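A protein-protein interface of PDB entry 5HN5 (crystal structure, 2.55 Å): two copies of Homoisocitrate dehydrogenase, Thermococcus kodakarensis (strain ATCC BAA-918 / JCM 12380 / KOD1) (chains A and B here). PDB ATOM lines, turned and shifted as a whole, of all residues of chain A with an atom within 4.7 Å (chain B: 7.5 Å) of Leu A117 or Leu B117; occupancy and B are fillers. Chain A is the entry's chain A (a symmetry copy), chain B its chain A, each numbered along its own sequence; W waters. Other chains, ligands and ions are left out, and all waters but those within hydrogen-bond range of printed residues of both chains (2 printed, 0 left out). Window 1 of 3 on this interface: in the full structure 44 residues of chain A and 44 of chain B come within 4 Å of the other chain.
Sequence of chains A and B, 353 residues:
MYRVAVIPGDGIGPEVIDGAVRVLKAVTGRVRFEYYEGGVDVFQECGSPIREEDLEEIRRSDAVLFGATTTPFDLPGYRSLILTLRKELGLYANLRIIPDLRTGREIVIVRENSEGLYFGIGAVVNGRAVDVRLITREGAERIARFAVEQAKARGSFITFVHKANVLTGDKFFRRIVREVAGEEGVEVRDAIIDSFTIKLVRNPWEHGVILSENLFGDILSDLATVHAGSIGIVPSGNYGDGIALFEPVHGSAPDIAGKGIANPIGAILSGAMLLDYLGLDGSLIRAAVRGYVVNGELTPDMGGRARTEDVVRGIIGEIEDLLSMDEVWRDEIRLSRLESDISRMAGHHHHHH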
ATOM      1  N   GLU A 115      26.418 -11.006 -34.670  1.00  0.00           N
ATOM      2  CA  GLU A 115      25.649 -11.628 -33.574  1.00  0.00           C
ATOM      3  C   GLU A 115      26.104 -11.130 -32.190  1.00  0.00           C
ATOM      4  O   GLU A 115      26.438  -9.971 -32.060  1.00  0.00           O
ATOM      5  CB  GLU A 115      25.632 -13.163 -33.722  1.00  0.00           C
ATOM      6  CG  GLU A 115      26.972 -13.867 -33.580  1.00  0.00           C
ATOM      7  CD  GLU A 115      26.895 -15.375 -33.851  1.00  0.00           C
ATOM      8  OE1 GLU A 115      27.787 -16.121 -33.375  1.00  0.00           O
ATOM      9  OE2 GLU A 115      25.951 -15.811 -34.539  1.00  0.00           O
ATOM     10  N   GLY A 116      26.088 -11.975 -31.157  1.00  0.00           N
ATOM     11  CA  GLY A 116      26.360 -11.522 -29.788  1.00  0.00           C
ATOM     12  C   GLY A 116      25.206 -10.697 -29.256  1.00  0.00           C
ATOM     13  O   GLY A 116      24.040 -11.032 -29.463  1.00  0.00           O
ATOM     14  N   LEU A 117      25.514  -9.596 -28.583  1.00  0.00           N
ATOM     15  CA  LEU A 117      24.457  -8.728 -28.067  1.00  0.00           C
ATOM     16  C   LEU A 117      23.822  -7.845 -29.155  1.00  0.00           C
ATOM     17  O   LEU A 117      22.856  -7.154 -28.885  1.00  0.00           O
ATOM     18  CB  LEU A 117      24.972  -7.914 -26.873  1.00  0.00           C
ATOM     19  CG  LEU A 117      24.962  -8.621 -25.508  1.00  0.00           C
ATOM     20  CD1 LEU A 117      25.710  -7.836 -24.448  1.00  0.00           C
ATOM     21  CD2 LEU A 117      23.529  -8.855 -25.080  1.00  0.00           C
ATOM     22  N   TYR A 118      24.349  -7.902 -30.376  1.00  0.00           N
ATOM     23  CA  TYR A 118      23.762  -7.235 -31.565  1.00  0.00           C
ATOM     24  C   TYR A 118      22.774  -8.106 -32.361  1.00  0.00           C
ATOM     25  O   TYR A 118      22.185  -7.633 -33.322  1.00  0.00           O
ATOM     26  CB  TYR A 118      24.887  -6.779 -32.532  1.00  0.00           C
ATOM     27  CG  TYR A 118      25.668  -5.599 -32.021  1.00  0.00           C
ATOM     28  CD1 TYR A 118      26.557  -5.734 -30.961  1.00  0.00           C
ATOM     29  CD2 TYR A 118      25.488  -4.340 -32.562  1.00  0.00           C
ATOM     30  CE1 TYR A 118      27.258  -4.642 -30.460  1.00  0.00           C
ATOM     31  CE2 TYR A 118      26.210  -3.251 -32.093  1.00  0.00           C
ATOM     32  CZ  TYR A 118      27.080  -3.403 -31.042  1.00  0.00           C
ATOM     33  OH  TYR A 118      27.766  -2.316 -30.579  1.00  0.00           O
ATOM     34  N   PHE A 119      22.590  -9.370 -32.002  1.00  0.00           N
ATOM     35  CA  PHE A 119      21.636 -10.216 -32.752  1.00  0.00           C
ATOM     36  C   PHE A 119      20.207  -9.644 -32.750  1.00  0.00           C
ATOM     37  O   PHE A 119      19.495  -9.789 -33.716  1.00  0.00           O
ATOM     38  CB  PHE A 119      21.639 -11.672 -32.252  1.00  0.00           C
ATOM     39  CG  PHE A 119      20.876 -12.624 -33.141  1.00  0.00           C
ATOM     40  CD1 PHE A 119      21.421 -13.058 -34.357  1.00  0.00           C
ATOM     41  CD2 PHE A 119      19.616 -13.092 -32.768  1.00  0.00           C
ATOM     42  CE1 PHE A 119      20.722 -13.929 -35.181  1.00  0.00           C
ATOM     43  CE2 PHE A 119      18.910 -13.966 -33.588  1.00  0.00           C
ATOM     44  CZ  PHE A 119      19.462 -14.381 -34.795  1.00  0.00           C
ATOM     45  N   GLY A 120      19.789  -9.009 -31.672  1.00  0.00           N
ATOM     46  CA  GLY A 120      18.581  -8.214 -31.697  1.00  0.00           C
ATOM     47  C   GLY A 120      17.354  -8.863 -31.093  1.00  0.00           C
ATOM     48  O   GLY A 120      16.251  -8.428 -31.323  1.00  0.00           O
ATOM     49  N   ASP A 131      17.948  -8.965 -22.976  1.00  0.00           N
ATOM     50  CA  ASP A 131      18.640  -8.980 -24.273  1.00  0.00           C
ATOM     51  C   ASP A 131      19.370 -10.282 -24.317  1.00  0.00           C
ATOM     52  O   ASP A 131      19.974 -10.692 -23.331  1.00  0.00           O
ATOM     53  CB  ASP A 131      19.674  -7.868 -24.411  1.00  0.00           C
ATOM     54  CG  ASP A 131      19.071  -6.471 -24.344  1.00  0.00           C
ATOM     55  OD1 ASP A 131      18.677  -5.929 -25.402  1.00  0.00           O
ATOM     56  OD2 ASP A 131      19.034  -5.911 -23.223  1.00  0.00           O
ATOM     57  N   VAL A 132      19.336 -10.928 -25.460  1.00  0.00           N
ATOM     58  CA  VAL A 132      19.898 -12.235 -25.586  1.00  0.00           C
ATOM     59  C   VAL A 132      21.231 -12.128 -26.279  1.00  0.00           C
ATOM     60  O   VAL A 132      21.283 -11.696 -27.404  1.00  0.00           O
ATOM     61  CB  VAL A 132      18.976 -13.135 -26.424  1.00  0.00           C
ATOM     62  CG1 VAL A 132      19.636 -14.485 -26.642  1.00  0.00           C
ATOM     63  CG2 VAL A 132      17.631 -13.304 -25.714  1.00  0.00           C
ATOM     64  N   ARG A 133      22.300 -12.540 -25.609  1.00  0.00           N
ATOM     65  CA  ARG A 133      23.607 -12.613 -26.231  1.00  0.00           C
ATOM     66  C   ARG A 133      23.667 -13.977 -26.921  1.00  0.00           C
ATOM     67  O   ARG A 133      23.702 -14.983 -26.257  1.00  0.00           O
ATOM     68  CB  ARG A 133      24.736 -12.430 -25.186  1.00  0.00           C
ATOM     69  CG  ARG A 133      26.030 -11.925 -25.789  1.00  0.00           C
ATOM     70  CD  ARG A 133      27.141 -11.584 -24.773  1.00  0.00           C
ATOM     71  NE  ARG A 133      27.964 -12.758 -24.679  1.00  0.00           N
ATOM     72  CZ  ARG A 133      29.263 -12.888 -24.885  1.00  0.00           C
ATOM     73  NH1 ARG A 133      30.091 -11.878 -25.107  1.00  0.00           N
ATOM     74  NH2 ARG A 133      29.748 -14.112 -24.779  1.00  0.00           N
ATOM     75  N   VAL A 166      31.683 -16.520 -16.650  1.00  0.00           N
ATOM     76  CA  VAL A 166      30.325 -16.075 -16.343  1.00  0.00           C
ATOM     77  C   VAL A 166      29.346 -16.330 -17.471  1.00  0.00           C
ATOM     78  O   VAL A 166      28.149 -16.492 -17.200  1.00  0.00           O
ATOM     79  CB  VAL A 166      30.340 -14.562 -16.089  1.00  0.00           C
ATOM     80  CG1 VAL A 166      28.938 -13.982 -16.084  1.00  0.00           C
ATOM     81  CG2 VAL A 166      31.068 -14.264 -14.786  1.00  0.00           C
ATOM     82  N   LEU A 167      29.839 -16.297 -18.720  1.00  0.00           N
ATOM     83  CA  LEU A 167      28.986 -16.306 -19.901  1.00  0.00           C
ATOM     84  C   LEU A 167      29.056 -17.612 -20.693  1.00  0.00           C
ATOM     85  O   LEU A 167      30.018 -17.866 -21.409  1.00  0.00           O
ATOM     86  CB  LEU A 167      29.379 -15.138 -20.832  1.00  0.00           C
ATOM     87  CG  LEU A 167      29.221 -13.728 -20.281  1.00  0.00           C
ATOM     88  CD1 LEU A 167      29.553 -12.708 -21.362  1.00  0.00           C
ATOM     89  CD2 LEU A 167      27.809 -13.474 -19.767  1.00  0.00           C
ATOM     90  N   GLU A 213      33.812 -11.159 -29.071  1.00  0.00           N
ATOM     91  CA  GLU A 213      32.411 -10.958 -29.365  1.00  0.00           C
ATOM     92  C   GLU A 213      32.125  -9.494 -29.750  1.00  0.00           C
ATOM     93  O   GLU A 213      32.911  -8.601 -29.454  1.00  0.00           O
ATOM     94  CB  GLU A 213      31.609 -11.398 -28.121  1.00  0.00           C
ATOM     95  CG  GLU A 213      30.096 -11.230 -28.135  1.00  0.00           C
ATOM     96  CD  GLU A 213      29.659  -9.828 -27.793  1.00  0.00           C
ATOM     97  OE1 GLU A 213      28.541  -9.440 -28.188  1.00  0.00           O
ATOM     98  OE2 GLU A 213      30.424  -9.104 -27.122  1.00  0.00           O
ATOM     99  N   LEU A 215      29.967  -6.854 -28.963  1.00  0.00           N
ATOM    100  CA  LEU A 215      29.950  -5.721 -28.065  1.00  0.00           C
ATOM    101  C   LEU A 215      31.283  -5.558 -27.352  1.00  0.00           C
ATOM    102  O   LEU A 215      31.737  -4.443 -27.160  1.00  0.00           O
ATOM    103  CB  LEU A 215      28.816  -5.855 -27.059  1.00  0.00           C
ATOM    104  CG  LEU A 215      28.714  -4.664 -26.117  1.00  0.00           C
ATOM    105  CD1 LEU A 215      28.332  -3.422 -26.892  1.00  0.00           C
ATOM    106  CD2 LEU A 215      27.722  -4.977 -25.015  1.00  0.00           C
ATOM    107  N   ARG B  79      31.499 -22.727  -9.378  1.00  0.00           N
ATOM    108  CA  ARG B  79      31.204 -21.307  -9.491  1.00  0.00           C
ATOM    109  C   ARG B  79      32.100 -20.508  -8.526  1.00  0.00           C
ATOM    110  O   ARG B  79      32.411 -20.954  -7.411  1.00  0.00           O
ATOM    111  CB  ARG B  79      29.711 -21.064  -9.252  1.00  0.00           C
ATOM    112  CG  ARG B  79      29.214 -19.727  -9.790  1.00  0.00           C
ATOM    113  CD  ARG B  79      27.781 -19.786 -10.320  1.00  0.00           C
ATOM    114  NE  ARG B  79      27.493 -18.653 -11.209  1.00  0.00           N
ATOM    115  CZ  ARG B  79      26.823 -17.549 -10.876  1.00  0.00           C
ATOM    116  NH1 ARG B  79      26.323 -17.389  -9.653  1.00  0.00           N
ATOM    117  NH2 ARG B  79      26.642 -16.592 -11.792  1.00  0.00           N
ATOM    118  N   GLU B 112      26.052  -2.351 -10.675  1.00  0.00           N
ATOM    119  CA  GLU B 112      24.920  -3.211 -10.262  1.00  0.00           C
ATOM    120  C   GLU B 112      25.432  -4.665 -10.176  1.00  0.00           C
ATOM    121  O   GLU B 112      26.150  -5.111 -11.052  1.00  0.00           O
ATOM    122  CB  GLU B 112      23.731  -3.092 -11.199  1.00  0.00           C
ATOM    123  CG  GLU B 112      22.443  -3.684 -10.644  1.00  0.00           C
ATOM    124  CD  GLU B 112      22.468  -5.204 -10.594  1.00  0.00           C
ATOM    125  OE1 GLU B 112      21.900  -5.781  -9.650  1.00  0.00           O
ATOM    126  OE2 GLU B 112      23.072  -5.844 -11.484  1.00  0.00           O
ATOM    127  N   SER B 114      23.749  -7.849  -8.915  1.00  0.00           N
ATOM    128  CA  SER B 114      22.850  -8.983  -8.748  1.00  0.00           C
ATOM    129  C   SER B 114      22.252  -9.506 -10.056  1.00  0.00           C
ATOM    130  O   SER B 114      21.728 -10.637 -10.085  1.00  0.00           O
ATOM    131  CB  SER B 114      21.697  -8.586  -7.835  1.00  0.00           C
ATOM    132  OG  SER B 114      20.743  -7.804  -8.543  1.00  0.00           O
ATOM    133  N   GLU B 115      22.310  -8.712 -11.130  1.00  0.00           N
ATOM    134  CA  GLU B 115      21.628  -9.096 -12.382  1.00  0.00           C
ATOM    135  C   GLU B 115      22.444  -8.712 -13.630  1.00  0.00           C
ATOM    136  O   GLU B 115      23.653  -8.802 -13.595  1.00  0.00           O
ATOM    137  CB  GLU B 115      20.174  -8.581 -12.390  1.00  0.00           C
ATOM    138  CG  GLU B 115      19.996  -7.071 -12.409  1.00  0.00           C
ATOM    139  CD  GLU B 115      18.530  -6.633 -12.303  1.00  0.00           C
ATOM    140  OE1 GLU B 115      18.208  -5.491 -12.717  1.00  0.00           O
ATOM    141  OE2 GLU B 115      17.705  -7.423 -11.803  1.00  0.00           O
ATOM    142  N   GLY B 116      21.801  -8.324 -14.733  1.00  0.00           N
ATOM    143  CA  GLY B 116      22.511  -8.097 -15.997  1.00  0.00           C
ATOM    144  C   GLY B 116      22.961  -9.410 -16.604  1.00  0.00           C
ATOM    145  O   GLY B 116      22.223 -10.395 -16.601  1.00  0.00           O
ATOM    146  N   LEU B 117      24.185  -9.449 -17.113  1.00  0.00           N
ATOM    147  CA  LEU B 117      24.706 -10.688 -17.687  1.00  0.00           C
ATOM    148  C   LEU B 117      25.154 -11.701 -16.619  1.00  0.00           C
ATOM    149  O   LEU B 117      25.507 -12.817 -16.954  1.00  0.00           O
ATOM    150  CB  LEU B 117      25.809 -10.381 -18.708  1.00  0.00           C
ATOM    151  CG  LEU B 117      25.344 -10.002 -20.124  1.00  0.00           C
ATOM    152  CD1 LEU B 117      26.480  -9.482 -20.982  1.00  0.00           C
ATOM    153  CD2 LEU B 117      24.700 -11.209 -20.773  1.00  0.00           C
ATOM    154  N   TYR B 118      25.106 -11.312 -15.346  1.00  0.00           N
ATOM    155  CA  TYR B 118      25.356 -12.213 -14.193  1.00  0.00           C
ATOM    156  C   TYR B 118      24.096 -12.900 -13.638  1.00  0.00           C
ATOM    157  O   TYR B 118      24.197 -13.712 -12.729  1.00  0.00           O
ATOM    158  CB  TYR B 118      26.024 -11.425 -13.035  1.00  0.00           C
ATOM    159  CG  TYR B 118      27.459 -11.069 -13.308  1.00  0.00           C
ATOM    160  CD1 TYR B 118      27.789 -10.089 -14.239  1.00  0.00           C
ATOM    161  CD2 TYR B 118      28.491 -11.738 -12.677  1.00  0.00           C
ATOM    162  CE1 TYR B 118      29.113  -9.776 -14.522  1.00  0.00           C
ATOM    163  CE2 TYR B 118      29.815 -11.407 -12.927  1.00  0.00           C
ATOM    164  CZ  TYR B 118      30.121 -10.440 -13.852  1.00  0.00           C
ATOM    165  OH  TYR B 118      31.431 -10.144 -14.101  1.00  0.00           O
ATOM    166  N   PHE B 119      22.910 -12.586 -14.144  1.00  0.00           N
ATOM    167  CA  PHE B 119      21.692 -13.246 -13.625  1.00  0.00           C
ATOM    168  C   PHE B 119      21.737 -14.777 -13.775  1.00  0.00           C
ATOM    169  O   PHE B 119      21.222 -15.483 -12.940  1.00  0.00           O
ATOM    170  CB  PHE B 119      20.411 -12.676 -14.263  1.00  0.00           C
ATOM    171  CG  PHE B 119      19.140 -13.134 -13.591  1.00  0.00           C
ATOM    172  CD1 PHE B 119      18.747 -12.594 -12.359  1.00  0.00           C
ATOM    173  CD2 PHE B 119      18.329 -14.101 -14.185  1.00  0.00           C
ATOM    174  CE1 PHE B 119      17.582 -13.016 -11.734  1.00  0.00           C
ATOM    175  CE2 PHE B 119      17.159 -14.528 -13.566  1.00  0.00           C
ATOM    176  CZ  PHE B 119      16.789 -13.988 -12.339  1.00  0.00           C
ATOM    177  N   GLY B 120      22.339 -15.284 -14.834  1.00  0.00           N
ATOM    178  CA  GLY B 120      22.663 -16.693 -14.904  1.00  0.00           C
ATOM    179  C   GLY B 120      21.729 -17.542 -15.739  1.00  0.00           C
ATOM    180  O   GLY B 120      21.725 -18.744 -15.627  1.00  0.00           O
ATOM    181  N   ILE B 121      20.935 -16.927 -16.592  1.00  0.00           N
ATOM    182  CA  ILE B 121      20.190 -17.685 -17.563  1.00  0.00           C
ATOM    183  C   ILE B 121      21.060 -17.817 -18.789  1.00  0.00           C
ATOM    184  O   ILE B 121      21.247 -16.866 -19.537  1.00  0.00           O
ATOM    185  CB  ILE B 121      18.869 -17.000 -17.913  1.00  0.00           C
ATOM    186  CG1 ILE B 121      17.948 -17.013 -16.687  1.00  0.00           C
ATOM    187  CG2 ILE B 121      18.212 -17.700 -19.097  1.00  0.00           C
ATOM    188  CD1 ILE B 121      16.862 -15.955 -16.725  1.00  0.00           C
ATOM    189  N   VAL B 130      23.455 -18.989 -25.739  1.00  0.00           N
ATOM    190  CA  VAL B 130      22.699 -17.834 -25.401  1.00  0.00           C
ATOM    191  C   VAL B 130      23.012 -17.446 -23.949  1.00  0.00           C
ATOM    192  O   VAL B 130      23.348 -18.296 -23.143  1.00  0.00           O
ATOM    193  CB  VAL B 130      21.224 -18.176 -25.689  1.00  0.00           C
ATOM    194  CG1 VAL B 130      20.283 -17.614 -24.658  1.00  0.00           C
ATOM    195  CG2 VAL B 130      20.872 -17.734 -27.109  1.00  0.00           C
ATOM    196  N   ASP B 131      23.000 -16.147 -23.656  1.00  0.00           N
ATOM    197  CA  ASP B 131      23.036 -15.627 -22.281  1.00  0.00           C
ATOM    198  C   ASP B 131      22.067 -14.490 -22.262  1.00  0.00           C
ATOM    199  O   ASP B 131      22.033 -13.685 -23.188  1.00  0.00           O
ATOM    200  CB  ASP B 131      24.401 -15.075 -21.886  1.00  0.00           C
ATOM    201  CG  ASP B 131      25.503 -16.126 -21.900  1.00  0.00           C
ATOM    202  OD1 ASP B 131      25.722 -16.790 -20.861  1.00  0.00           O
ATOM    203  OD2 ASP B 131      26.172 -16.248 -22.954  1.00  0.00           O
ATOM    204  N   VAL B 132      21.292 -14.405 -21.206  1.00  0.00           N
ATOM    205  CA  VAL B 132      20.251 -13.431 -21.131  1.00  0.00           C
ATOM    206  C   VAL B 132      20.704 -12.299 -20.248  1.00  0.00           C
ATOM    207  O   VAL B 132      20.963 -12.516 -19.090  1.00  0.00           O
ATOM    208  CB  VAL B 132      18.981 -14.051 -20.528  1.00  0.00           C
ATOM    209  CG1 VAL B 132      17.919 -12.979 -20.352  1.00  0.00           C
ATOM    210  CG2 VAL B 132      18.467 -15.170 -21.437  1.00  0.00           C
ATOM    211  N   ARG B 133      20.781 -11.092 -20.795  1.00  0.00           N
ATOM    212  CA  ARG B 133      21.070  -9.913 -20.002  1.00  0.00           C
ATOM    213  C   ARG B 133      19.724  -9.441 -19.450  1.00  0.00           C
ATOM    214  O   ARG B 133      18.896  -8.985 -20.199  1.00  0.00           O
ATOM    215  CB  ARG B 133      21.774  -8.826 -20.851  1.00  0.00           C
ATOM    216  CG  ARG B 133      22.597  -7.863 -20.022  1.00  0.00           C
ATOM    217  CD  ARG B 133      23.438  -6.851 -20.829  1.00  0.00           C
ATOM    218  NE  ARG B 133      22.640  -5.659 -20.920  1.00  0.00           N
ATOM    219  CZ  ARG B 133      22.932  -4.426 -20.544  1.00  0.00           C
ATOM    220  NH1 ARG B 133      24.121  -4.038 -20.107  1.00  0.00           N
ATOM    221  NH2 ARG B 133      21.975  -3.530 -20.701  1.00  0.00           N
ATOM    222  N   LEU B 134      19.508  -9.571 -18.142  1.00  0.00           N
ATOM    223  CA  LEU B 134      18.229  -9.215 -17.534  1.00  0.00           C
ATOM    224  C   LEU B 134      18.374  -8.004 -16.682  1.00  0.00           C
ATOM    225  O   LEU B 134      19.193  -7.978 -15.775  1.00  0.00           O
ATOM    226  CB  LEU B 134      17.711 -10.347 -16.673  1.00  0.00           C
ATOM    227  CG  LEU B 134      16.484 -10.036 -15.831  1.00  0.00           C
ATOM    228  CD1 LEU B 134      15.231  -9.840 -16.673  1.00  0.00           C
ATOM    229  CD2 LEU B 134      16.286 -11.164 -14.848  1.00  0.00           C
ATOM    230  N   ILE B 135      17.607  -6.977 -16.998  1.00  0.00           N
ATOM    231  CA  ILE B 135      17.447  -5.832 -16.113  1.00  0.00           C
ATOM    232  C   ILE B 135      15.998  -5.817 -15.667  1.00  0.00           C
ATOM    233  O   ILE B 135      15.084  -6.054 -16.466  1.00  0.00           O
ATOM    234  CB  ILE B 135      17.707  -4.497 -16.796  1.00  0.00           C
ATOM    235  CG1 ILE B 135      19.022  -4.513 -17.605  1.00  0.00           C
ATOM    236  CG2 ILE B 135      17.672  -3.401 -15.761  1.00  0.00           C
ATOM    237  CD1 ILE B 135      20.305  -4.742 -16.827  1.00  0.00           C
ATOM    238  N   VAL B 166      21.561  -0.067 -28.668  1.00  0.00           N
ATOM    239  CA  VAL B 166      21.557  -1.457 -29.120  1.00  0.00           C
ATOM    240  C   VAL B 166      20.824  -2.387 -28.175  1.00  0.00           C
ATOM    241  O   VAL B 166      20.306  -3.416 -28.630  1.00  0.00           O
ATOM    242  CB  VAL B 166      23.004  -1.956 -29.218  1.00  0.00           C
ATOM    243  CG1 VAL B 166      23.067  -3.465 -29.366  1.00  0.00           C
ATOM    244  CG2 VAL B 166      23.715  -1.256 -30.367  1.00  0.00           C
ATOM    245  N   LEU B 167      20.844  -2.066 -26.871  1.00  0.00           N
ATOM    246  CA  LEU B 167      20.376  -2.973 -25.831  1.00  0.00           C
ATOM    247  C   LEU B 167      19.073  -2.521 -25.171  1.00  0.00           C
ATOM    248  O   LEU B 167      19.062  -1.608 -24.354  1.00  0.00           O
ATOM    249  CB  LEU B 167      21.462  -3.115 -24.743  1.00  0.00           C
ATOM    250  CG  LEU B 167      22.797  -3.709 -25.168  1.00  0.00           C
ATOM    251  CD1 LEU B 167      23.703  -3.871 -23.954  1.00  0.00           C
ATOM    252  CD2 LEU B 167      22.627  -5.060 -25.850  1.00  0.00           C
ATOM    253  N   THR B 168      17.981  -3.202 -25.472  1.00  0.00           N
ATOM    254  CA  THR B 168      16.683  -2.816 -24.928  1.00  0.00           C
ATOM    255  C   THR B 168      16.667  -2.748 -23.400  1.00  0.00           C
ATOM    256  O   THR B 168      15.971  -1.933 -22.820  1.00  0.00           O
ATOM    257  CB  THR B 168      15.556  -3.760 -25.365  1.00  0.00           C
ATOM    258  OG1 THR B 168      15.368  -4.763 -24.379  1.00  0.00           O
ATOM    259  CG2 THR B 168      15.827  -4.402 -26.701  1.00  0.00           C
ATOM    260  N   GLU B 213      25.488  -1.229 -15.598  1.00  0.00           N
ATOM    261  CA  GLU B 213      25.156  -2.633 -15.490  1.00  0.00           C
ATOM    262  C   GLU B 213      26.363  -3.457 -15.006  1.00  0.00           C
ATOM    263  O   GLU B 213      27.503  -3.015 -15.097  1.00  0.00           O
ATOM    264  CB  GLU B 213      24.651  -3.098 -16.874  1.00  0.00           C
ATOM    265  CG  GLU B 213      24.290  -4.564 -17.060  1.00  0.00           C
ATOM    266  CD  GLU B 213      25.494  -5.435 -17.320  1.00  0.00           C
ATOM    267  OE1 GLU B 213      25.417  -6.652 -17.053  1.00  0.00           O
ATOM    268  OE2 GLU B 213      26.524  -4.915 -17.800  1.00  0.00           O
ATOM    269  N   ASN B 214      26.067  -4.652 -14.497  1.00  0.00           N
ATOM    270  CA  ASN B 214      27.018  -5.571 -13.851  1.00  0.00           C
ATOM    271  C   ASN B 214      28.310  -5.754 -14.643  1.00  0.00           C
ATOM    272  O   ASN B 214      29.387  -5.349 -14.202  1.00  0.00           O
ATOM    273  CB  ASN B 214      26.338  -6.924 -13.600  1.00  0.00           C
ATOM    274  CG  ASN B 214      26.812  -7.631 -12.311  1.00  0.00           C
ATOM    275  OD1 ASN B 214      28.002  -7.717 -11.994  1.00  0.00           O
ATOM    276  ND2 ASN B 214      25.856  -8.156 -11.576  1.00  0.00           N
ATOM    277  N   LEU B 215      28.195  -6.323 -15.828  1.00  0.00           N
ATOM    278  CA  LEU B 215      29.371  -6.653 -16.602  1.00  0.00           C
ATOM    279  C   LEU B 215      30.078  -5.401 -17.097  1.00  0.00           C
ATOM    280  O   LEU B 215      31.296  -5.357 -17.110  1.00  0.00           O
ATOM    281  CB  LEU B 215      29.004  -7.560 -17.769  1.00  0.00           C
ATOM    282  CG  LEU B 215      30.211  -7.984 -18.592  1.00  0.00           C
ATOM    283  CD1 LEU B 215      31.124  -8.858 -17.762  1.00  0.00           C
ATOM    284  CD2 LEU B 215      29.741  -8.685 -19.852  1.00  0.00           C
ATOM    285  N   PHE B 216      29.312  -4.398 -17.497  1.00  0.00           N
ATOM    286  CA  PHE B 216      29.879  -3.104 -17.860  1.00  0.00           C
ATOM    287  C   PHE B 216      30.679  -2.542 -16.721  1.00  0.00           C
ATOM    288  O   PHE B 216      31.804  -2.133 -16.922  1.00  0.00           O
ATOM    289  CB  PHE B 216      28.795  -2.096 -18.261  1.00  0.00           C
ATOM    290  CG  PHE B 216      28.220  -2.321 -19.632  1.00  0.00           C
ATOM    291  CD1 PHE B 216      28.869  -3.118 -20.582  1.00  0.00           C
ATOM    292  CD2 PHE B 216      27.052  -1.694 -19.990  1.00  0.00           C
ATOM    293  CE1 PHE B 216      28.318  -3.307 -21.848  1.00  0.00           C
ATOM    294  CE2 PHE B 216      26.505  -1.869 -21.249  1.00  0.00           C
ATOM    295  CZ  PHE B 216      27.139  -2.677 -22.179  1.00  0.00           C
HETATM  296  O   HOH W   1      25.502 -15.500 -16.346  1.00  0.00           O
HETATM  297  O   HOH W   2      20.448  -6.144 -29.751  1.00  0.00           O
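O of Asp B131 lies within hydrogen-bond range of N of Arg A133 (2.7 Å).
N of Arg B133 sits at hydrogen-bond distance from O of Asp A131, 2.7 Å away.
OD1 of Asp A131 lies within hydrogen-bond range of N of Thr B168 (2.8 Å).
The backbone carbonyl oxygen (O) of Ile B121 sits at hydrogen-bond distance from the backbone NH (N) of Val B132, 3.0 Å away.
The guanidinium group (NH1) of Arg A133 is in salt-bridge range of the side-chain carboxylate (OE2) of Glu A213 (3.4 Å).
The backbone NH (N) of Phe B216 lies within hydrogen-bond range of the side-chain carboxylate (OE2) of Glu B213 (2.9 Å).
The side-chain carboxylate (OE2) of Glu A213 sits at hydrogen-bond distance from the backbone NH (N) of Leu A215, at 2.9 Å.
The guanidinium group (NH1) of Arg B133 is in salt-bridge range of the side-chain carboxylate (OE2) of Glu B213, at 3.4 Å.
Leu A117 touches Val B166, and with the chains exchanged Val A166 touches Leu B117.
Asp B131 touches its own counterpart, Asp A131.
Asp A131 touches Val B132, and with the chains exchanged Val A132 touches Asp B131.
Asp A131 touches Leu B167, and with the chains exchanged Leu A167 touches Asp B131.
13 positions are printed for both chains.
Of the 18 pairs that touch across the chains among the printed residues, 14 have their exchanged pair printed and touching as well.
Water W1 bridges the backbone carbonyl oxygen of Leu B117 and the backbone carbonyl oxygen of Val A166.
Water W2 lies within hydrogen-bond range of O of Leu A117 (2.8 Å) and O of Val B166 (3.0 Å).
Leu A117 touches three residues of chain B.
Of chain A, only Leu A117, Val A166 and Leu A167 come within 4 Å of Leu B117.
Printed residues of chain B within 4 Å of Val A132: Val B130 (3.5 Å) and Asp B131 (3.5 Å).
Of the printed residues of chain A, Val B166 touches Leu A117 (3.7 Å) and Tyr A118 (3.6 Å).
Of the printed residues of chain B, Val A166 touches Leu B117 and Tyr B118.
Printed residues of chain A within 4 Å of Asp B131: Asp A131 (3.6 Å), Val A132 (3.5 Å), Arg A133 (2.7 Å) and Leu A167 (3.4 Å).
Arg B79 touches none of the printed residues of chain A.
Glu A115 touches none of the printed residues of chain B.
The nearest residue of chain B that does not touch Leu A117 is Arg B133 (4.4 Å).
Leu B117 touches Leu A117.
Leu A117 touches Val B166 (O to CG1, 3.7 Å).
Tyr A118 touches Val B166.
O of Asp B131 touches O of Asp A131 (3.6 Å).
Asp A131 touches Val B132.
OD1 of Asp A131 touches CA of Leu B167 (3.4 Å).
Val A132 touches Val B130.
Asp B131 touches Val A132 (O to CA, 3.5 Å).
Val A166 touches Tyr B118 (CG2 to CE2, 3.6 Å).
Leu A215 touches Phe B216.
Of the 13 printed residues of chain A, 8 touch a printed residue of chain B.
Hydrophobic or aromatic side chains of chain A that line the printed part of chain B: Leu A117, Tyr A118, Val A132, Val A166, Leu A167 and Leu A215.
Hydrophobic or aromatic side chains of chain B that line the printed part of chain A: Leu B117, Tyr B118, Val B130, Val B166, Leu B167 and Phe B216.
Among the printed residues, 18 pairs touch across the chains.
Among the printed residues, no Asp or Glu carboxylate lies within 4 Å of a Lys or Arg side-chain nitrogen of the other chain.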
